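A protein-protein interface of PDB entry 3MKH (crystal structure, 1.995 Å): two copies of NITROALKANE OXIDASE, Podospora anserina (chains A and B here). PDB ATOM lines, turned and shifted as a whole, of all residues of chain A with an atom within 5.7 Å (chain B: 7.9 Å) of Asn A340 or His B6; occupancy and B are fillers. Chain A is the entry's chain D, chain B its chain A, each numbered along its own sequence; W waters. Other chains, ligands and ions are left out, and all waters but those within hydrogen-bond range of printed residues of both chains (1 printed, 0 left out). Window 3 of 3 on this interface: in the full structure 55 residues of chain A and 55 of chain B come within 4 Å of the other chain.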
ATOM      1  N   ALA A   2     -10.938   0.289  14.297  1.00  0.00           N
ATOM      2  CA  ALA A   2     -11.035   1.679  13.831  1.00  0.00           C
ATOM      3  C   ALA A   2     -12.508   2.059  13.707  1.00  0.00           C
ATOM      4  O   ALA A   2     -13.206   1.533  12.838  1.00  0.00           O
ATOM      5  CB  ALA A   2     -10.340   1.824  12.497  1.00  0.00           C
ATOM      6  N   ILE A   3     -12.988   2.951  14.572  1.00  0.00           N
ATOM      7  CA  ILE A   3     -14.424   3.220  14.642  1.00  0.00           C
ATOM      8  C   ILE A   3     -14.999   3.595  13.278  1.00  0.00           C
ATOM      9  O   ILE A   3     -14.552   4.554  12.632  1.00  0.00           O
ATOM     10  CB  ILE A   3     -14.767   4.275  15.724  1.00  0.00           C
ATOM     11  CG1 ILE A   3     -14.425   3.700  17.101  1.00  0.00           C
ATOM     12  CG2 ILE A   3     -16.253   4.642  15.665  1.00  0.00           C
ATOM     13  CD1 ILE A   3     -14.084   4.749  18.137  1.00  0.00           C
ATOM     14  N   ILE A  76     -24.521  -8.492  13.206  1.00  0.00           N
ATOM     15  CA  ILE A  76     -24.728  -7.188  12.589  1.00  0.00           C
ATOM     16  C   ILE A  76     -25.562  -7.326  11.320  1.00  0.00           C
ATOM     17  O   ILE A  76     -26.476  -6.547  11.092  1.00  0.00           O
ATOM     18  CB  ILE A  76     -23.413  -6.470  12.271  1.00  0.00           C
ATOM     19  CG1 ILE A  76     -22.718  -6.035  13.560  1.00  0.00           C
ATOM     20  CG2 ILE A  76     -23.674  -5.256  11.393  1.00  0.00           C
ATOM     21  CD1 ILE A  76     -21.248  -5.703  13.365  1.00  0.00           C
ATOM     22  N   ALA A 335     -24.474  -5.686  18.760  1.00  0.00           N
ATOM     23  CA  ALA A 335     -24.301  -6.747  17.765  1.00  0.00           C
ATOM     24  C   ALA A 335     -22.820  -6.960  17.538  1.00  0.00           C
ATOM     25  O   ALA A 335     -22.346  -8.090  17.472  1.00  0.00           O
ATOM     26  CB  ALA A 335     -25.007  -6.388  16.449  1.00  0.00           C
ATOM     27  N   HIS A 336     -22.081  -5.861  17.437  1.00  0.00           N
ATOM     28  CA  HIS A 336     -20.649  -5.939  17.218  1.00  0.00           C
ATOM     29  C   HIS A 336     -19.915  -6.515  18.421  1.00  0.00           C
ATOM     30  O   HIS A 336     -19.083  -7.419  18.276  1.00  0.00           O
ATOM     31  CB  HIS A 336     -20.077  -4.571  16.858  1.00  0.00           C
ATOM     32  CG  HIS A 336     -18.627  -4.611  16.489  1.00  0.00           C
ATOM     33  ND1 HIS A 336     -17.620  -4.483  17.421  1.00  0.00           N
ATOM     34  CD2 HIS A 336     -18.014  -4.790  15.295  1.00  0.00           C
ATOM     35  CE1 HIS A 336     -16.449  -4.555  16.812  1.00  0.00           C
ATOM     36  NE2 HIS A 336     -16.659  -4.740  15.523  1.00  0.00           N
ATOM     37  N   ALA A 337     -20.231  -6.007  19.609  1.00  0.00           N
ATOM     38  CA  ALA A 337     -19.539  -6.422  20.822  1.00  0.00           C
ATOM     39  C   ALA A 337     -19.780  -7.892  21.171  1.00  0.00           C
ATOM     40  O   ALA A 337     -18.883  -8.572  21.678  1.00  0.00           O
ATOM     41  CB  ALA A 337     -19.944  -5.533  21.997  1.00  0.00           C
ATOM     42  N   MET A 338     -20.993  -8.373  20.932  1.00  0.00           N
ATOM     43  CA  MET A 338     -21.320  -9.764  21.231  1.00  0.00           C
ATOM     44  C   MET A 338     -20.351 -10.746  20.562  1.00  0.00           C
ATOM     45  O   MET A 338     -20.019 -11.789  21.126  1.00  0.00           O
ATOM     46  CB  MET A 338     -22.745 -10.089  20.802  1.00  0.00           C
ATOM     47  CG  MET A 338     -23.811  -9.730  21.837  1.00  0.00           C
ATOM     48  SD  MET A 338     -23.668 -10.726  23.339  1.00  0.00           S
ATOM     49  CE  MET A 338     -23.860 -12.367  22.643  1.00  0.00           C
ATOM     50  N   GLU A 339     -19.906 -10.406  19.359  1.00  0.00           N
ATOM     51  CA  GLU A 339     -19.054 -11.301  18.585  1.00  0.00           C
ATOM     52  C   GLU A 339     -17.590 -10.865  18.542  1.00  0.00           C
ATOM     53  O   GLU A 339     -16.725 -11.623  18.096  1.00  0.00           O
ATOM     54  CB  GLU A 339     -19.624 -11.471  17.168  1.00  0.00           C
ATOM     55  CG  GLU A 339     -21.037 -12.071  17.166  1.00  0.00           C
ATOM     56  CD  GLU A 339     -21.536 -12.452  15.779  1.00  0.00           C
ATOM     57  OE1 GLU A 339     -21.148 -11.786  14.792  1.00  0.00           O
ATOM     58  OE2 GLU A 339     -22.323 -13.423  15.682  1.00  0.00           O
ATOM     59  N   ASN A 340     -17.302  -9.654  19.018  1.00  0.00           N
ATOM     60  CA  ASN A 340     -15.961  -9.106  18.869  1.00  0.00           C
ATOM     61  C   ASN A 340     -15.339  -8.520  20.132  1.00  0.00           C
ATOM     62  O   ASN A 340     -14.159  -8.176  20.127  1.00  0.00           O
ATOM     63  CB  ASN A 340     -15.940  -8.048  17.758  1.00  0.00           C
ATOM     64  CG  ASN A 340     -16.334  -8.607  16.416  1.00  0.00           C
ATOM     65  OD1 ASN A 340     -15.500  -9.147  15.695  1.00  0.00           O
ATOM     66  ND2 ASN A 340     -17.604  -8.463  16.057  1.00  0.00           N
ATOM     67  N   GLY A 341     -16.113  -8.393  21.205  1.00  0.00           N
ATOM     68  CA  GLY A 341     -15.603  -7.750  22.410  1.00  0.00           C
ATOM     69  C   GLY A 341     -15.453  -6.257  22.175  1.00  0.00           C
ATOM     70  O   GLY A 341     -15.997  -5.743  21.189  1.00  0.00           O
ATOM     71  N   PRO A 342     -14.665  -5.553  23.019  1.00  0.00           N
ATOM     72  CA  PRO A 342     -13.697  -6.007  24.033  1.00  0.00           C
ATOM     73  C   PRO A 342     -14.211  -6.435  25.408  1.00  0.00           C
ATOM     74  O   PRO A 342     -13.392  -6.612  26.320  1.00  0.00           O
ATOM     75  CB  PRO A 342     -12.831  -4.768  24.238  1.00  0.00           C
ATOM     76  CG  PRO A 342     -13.803  -3.646  24.044  1.00  0.00           C
ATOM     77  CD  PRO A 342     -14.613  -4.087  22.861  1.00  0.00           C
ATOM     78  N   ARG A 348     -20.315  -8.253  27.372  1.00  0.00           N
ATOM     79  CA  ARG A 348     -20.967  -8.318  26.074  1.00  0.00           C
ATOM     80  C   ARG A 348     -22.470  -8.428  26.196  1.00  0.00           C
ATOM     81  O   ARG A 348     -23.211  -7.701  25.524  1.00  0.00           O
ATOM     82  CB  ARG A 348     -20.421  -9.484  25.246  1.00  0.00           C
ATOM     83  CG  ARG A 348     -18.975  -9.301  24.851  1.00  0.00           C
ATOM     84  CD  ARG A 348     -18.356 -10.618  24.461  1.00  0.00           C
ATOM     85  NE  ARG A 348     -17.090 -10.426  23.772  1.00  0.00           N
ATOM     86  CZ  ARG A 348     -16.154 -11.363  23.674  1.00  0.00           C
ATOM     87  NH1 ARG A 348     -16.349 -12.551  24.243  1.00  0.00           N
ATOM     88  NH2 ARG A 348     -15.021 -11.114  23.024  1.00  0.00           N
ATOM     89  N   ILE B   3     -18.738  -1.969   9.536  1.00  0.00           N
ATOM     90  CA  ILE B   3     -19.220  -1.550  10.840  1.00  0.00           C
ATOM     91  C   ILE B   3     -18.300  -2.084  11.926  1.00  0.00           C
ATOM     92  O   ILE B   3     -18.161  -3.292  12.104  1.00  0.00           O
ATOM     93  CB  ILE B   3     -20.678  -1.993  11.065  1.00  0.00           C
ATOM     94  CG1 ILE B   3     -21.571  -1.384   9.970  1.00  0.00           C
ATOM     95  CG2 ILE B   3     -21.161  -1.602  12.481  1.00  0.00           C
ATOM     96  CD1 ILE B   3     -22.945  -2.004   9.867  1.00  0.00           C
ATOM     97  N   ASP B   4     -17.661  -1.172  12.648  1.00  0.00           N
ATOM     98  CA  ASP B   4     -16.611  -1.546  13.588  1.00  0.00           C
ATOM     99  C   ASP B   4     -16.632  -0.577  14.772  1.00  0.00           C
ATOM    100  O   ASP B   4     -16.540   0.632  14.574  1.00  0.00           O
ATOM    101  CB  ASP B   4     -15.252  -1.482  12.876  1.00  0.00           C
ATOM    102  CG  ASP B   4     -14.129  -2.128  13.680  1.00  0.00           C
ATOM    103  OD1 ASP B   4     -14.365  -2.545  14.841  1.00  0.00           O
ATOM    104  OD2 ASP B   4     -13.000  -2.206  13.144  1.00  0.00           O
ATOM    105  N   PHE B   5     -16.758  -1.107  15.990  1.00  0.00           N
ATOM    106  CA  PHE B   5     -16.748  -0.286  17.208  1.00  0.00           C
ATOM    107  C   PHE B   5     -15.440  -0.388  18.015  1.00  0.00           C
ATOM    108  O   PHE B   5     -15.334   0.143  19.126  1.00  0.00           O
ATOM    109  CB  PHE B   5     -17.956  -0.634  18.094  1.00  0.00           C
ATOM    110  CG  PHE B   5     -19.281  -0.175  17.523  1.00  0.00           C
ATOM    111  CD1 PHE B   5     -19.908  -0.897  16.518  1.00  0.00           C
ATOM    112  CD2 PHE B   5     -19.885   0.980  17.987  1.00  0.00           C
ATOM    113  CE1 PHE B   5     -21.115  -0.475  15.981  1.00  0.00           C
ATOM    114  CE2 PHE B   5     -21.097   1.409  17.461  1.00  0.00           C
ATOM    115  CZ  PHE B   5     -21.710   0.677  16.456  1.00  0.00           C
ATOM    116  N   HIS B   6     -14.436  -1.057  17.455  1.00  0.00           N
ATOM    117  CA  HIS B   6     -13.121  -1.115  18.096  1.00  0.00           C
ATOM    118  C   HIS B   6     -12.320   0.158  17.839  1.00  0.00           C
ATOM    119  O   HIS B   6     -12.268   0.655  16.718  1.00  0.00           O
ATOM    120  CB  HIS B   6     -12.319  -2.331  17.606  1.00  0.00           C
ATOM    121  CG  HIS B   6     -12.802  -3.634  18.161  1.00  0.00           C
ATOM    122  ND1 HIS B   6     -12.325  -4.853  17.730  1.00  0.00           N
ATOM    123  CD2 HIS B   6     -13.715  -3.907  19.124  1.00  0.00           C
ATOM    124  CE1 HIS B   6     -12.924  -5.821  18.400  1.00  0.00           C
ATOM    125  NE2 HIS B   6     -13.775  -5.274  19.250  1.00  0.00           N
ATOM    126  N   LEU B   7     -11.680   0.673  18.880  1.00  0.00           N
ATOM    127  CA  LEU B   7     -10.809   1.817  18.722  1.00  0.00           C
ATOM    128  C   LEU B   7      -9.526   1.353  18.051  1.00  0.00           C
ATOM    129  O   LEU B   7      -9.002   0.283  18.378  1.00  0.00           O
ATOM    130  CB  LEU B   7     -10.454   2.427  20.079  1.00  0.00           C
ATOM    131  CG  LEU B   7     -11.500   3.240  20.845  1.00  0.00           C
ATOM    132  CD1 LEU B   7     -12.689   2.391  21.184  1.00  0.00           C
ATOM    133  CD2 LEU B   7     -10.859   3.775  22.096  1.00  0.00           C
ATOM    134  N   SER B   8      -9.022   2.173  17.134  1.00  0.00           N
ATOM    135  CA  SER B   8      -7.718   1.965  16.523  1.00  0.00           C
ATOM    136  C   SER B   8      -6.636   2.274  17.549  1.00  0.00           C
ATOM    137  O   SER B   8      -6.931   2.775  18.629  1.00  0.00           O
ATOM    138  CB  SER B   8      -7.559   2.894  15.322  1.00  0.00           C
ATOM    139  OG  SER B   8      -7.550   4.257  15.724  1.00  0.00           O
ATOM    140  N   ALA B   9      -5.383   1.983  17.212  1.00  0.00           N
ATOM    141  CA  ALA B   9      -4.272   2.301  18.101  1.00  0.00           C
ATOM    142  C   ALA B   9      -4.231   3.801  18.398  1.00  0.00           C
ATOM    143  O   ALA B   9      -3.965   4.216  19.524  1.00  0.00           O
ATOM    144  CB  ALA B   9      -2.950   1.845  17.489  1.00  0.00           C
ATOM    145  N   GLN B  11      -6.799   5.809  18.399  1.00  0.00           N
ATOM    146  CA  GLN B  11      -7.948   6.152  19.224  1.00  0.00           C
ATOM    147  C   GLN B  11      -7.747   5.669  20.654  1.00  0.00           C
ATOM    148  O   GLN B  11      -8.146   6.343  21.605  1.00  0.00           O
ATOM    149  CB  GLN B  11      -9.236   5.607  18.607  1.00  0.00           C
ATOM    150  CG  GLN B  11      -9.580   6.298  17.279  1.00  0.00           C
ATOM    151  CD  GLN B  11     -10.638   5.566  16.482  1.00  0.00           C
ATOM    152  OE1 GLN B  11     -10.854   4.365  16.668  1.00  0.00           O
ATOM    153  NE2 GLN B  11     -11.310   6.287  15.589  1.00  0.00           N
ATOM    154  N   LYS B  12      -7.108   4.517  20.811  1.00  0.00           N
ATOM    155  CA  LYS B  12      -6.732   4.069  22.144  1.00  0.00           C
ATOM    156  C   LYS B  12      -5.745   5.046  22.754  1.00  0.00           C
ATOM    157  O   LYS B  12      -5.814   5.351  23.946  1.00  0.00           O
ATOM    158  CB  LYS B  12      -6.141   2.656  22.106  1.00  0.00           C
ATOM    159  CG  LYS B  12      -7.203   1.586  22.064  1.00  0.00           C
ATOM    160  CD  LYS B  12      -6.627   0.201  21.821  1.00  0.00           C
ATOM    161  CE  LYS B  12      -7.748  -0.789  21.512  1.00  0.00           C
ATOM    162  NZ  LYS B  12      -7.239  -2.139  21.159  1.00  0.00           N
ATOM    163  N   TRP B 332     -20.981   8.825  18.850  1.00  0.00           N
ATOM    164  CA  TRP B 332     -19.927   8.356  17.931  1.00  0.00           C
ATOM    165  C   TRP B 332     -20.433   8.236  16.487  1.00  0.00           C
ATOM    166  O   TRP B 332     -19.708   8.531  15.531  1.00  0.00           O
ATOM    167  CB  TRP B 332     -19.337   7.034  18.417  1.00  0.00           C
ATOM    168  CG  TRP B 332     -18.435   7.196  19.625  1.00  0.00           C
ATOM    169  CD1 TRP B 332     -18.294   8.313  20.408  1.00  0.00           C
ATOM    170  CD2 TRP B 332     -17.544   6.216  20.170  1.00  0.00           C
ATOM    171  NE1 TRP B 332     -17.373   8.083  21.410  1.00  0.00           N
ATOM    172  CE2 TRP B 332     -16.899   6.805  21.284  1.00  0.00           C
ATOM    173  CE3 TRP B 332     -17.224   4.898  19.822  1.00  0.00           C
ATOM    174  CZ2 TRP B 332     -15.958   6.118  22.055  1.00  0.00           C
ATOM    175  CZ3 TRP B 332     -16.294   4.214  20.594  1.00  0.00           C
ATOM    176  CH2 TRP B 332     -15.670   4.829  21.693  1.00  0.00           C
HETATM  177  O   HOH W   1     -12.603   6.533  13.153  1.00  0.00           O
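OD1 of Asp B4 lies within hydrogen-bond range of NE2 of His A336, at 3.2 Å. The side-chain carboxylate (OD2) of Asp B4 sits at hydrogen-bond distance from the backbone NH (N) of Ala A2 (3.4 Å). A ring nitrogen (NE2) of His B6 sits at hydrogen-bond distance from the backbone carbonyl oxygen of Gly A341 (3.0 Å). The side-chain amide oxygen (OE1) of Gln B11 lies within hydrogen-bond range of the backbone NH (N) of Ile A3. The backbone carbonyl oxygen (O) of His B6 lies within hydrogen-bond range of the backbone NH (N) of Ala A2 (2.8 Å). A ring nitrogen (NE2) of His B6 sits at hydrogen-bond distance from the backbone carbonyl oxygen (O) of Asn A340 (3.1 Å). The backbone NH (N) of Ile A3 is in hydrogen-bond range of the backbone carbonyl oxygen (O) of His B6, 3.2 Å away.
The backbone NH of Ser B8 sits at hydrogen-bond distance from the side-chain amide oxygen of Gln B11. OD1 of Asp B4 is in hydrogen-bond range of N of His B6, 3.0 Å away. O of His A336 lies within hydrogen-bond range of ND2 of Asn A340.
Ala A2 touches Ser B8. Ala A2 touches Gln B11. Ile A3 touches Asp B4 (CA to O, 3.3 Å). Trp B332 touches Ile A3 (CZ3 to CD1, 3.3 Å). CG2 of Ile A76 touches CD1 of Ile B3 (3.7 Å). O of Ile B3 touches CD2 of His A336, 3.5 Å away. His A336 touches Phe B5. His B6 touches His A336 (CD2 to CE1, 3.6 Å). Pro A342 touches His B6.
Of the printed residues of chain B, Ala A2 touches Asp B4, His B6, Ser B8 and Gln B11. Printed residues of chain B within 4 Å of Ile A3: Asp B4, His B6, Gln B11 and Trp B332. Asn A340 touches just one residue of chain B: His B6 (3.1 Å). Gly A341 touches just one residue of chain B: His B6. Of chain A, only Ala A2 (2.8 Å), Ile A3 (3.2 Å), His A336 (3.6 Å), Asn A340 (3.1 Å), Gly A341 (3.0 Å) and Pro A342 (3.8 Å) come within 4 Å of His B6. The nearest printed residue of chain A that does not touch His B6 is Ala A337 (6.1 Å). The nearest printed residue of chain A that does not touch Asp B4 is Ile A76 (5.8 Å).
Hydrophobic or aromatic side chains of chain B that line the printed part of chain A: Ile B3, Phe B5, His B6 and Trp B332. Along chain B the printed residues that touch a printed residue of chain A span positions 3 to 332. Of the 12 printed residues of chain A, 7 touch a printed residue of chain B. Hydrophobic or aromatic side chains of chain A that line the printed part of chain B: Ile A3, Ile A76, His A336 and Pro A342.
1 position is printed for both chains.
Water W1 bridges NE2 of Gln B11 (2.8 Å) and O of Ile A3 (2.8 Å).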
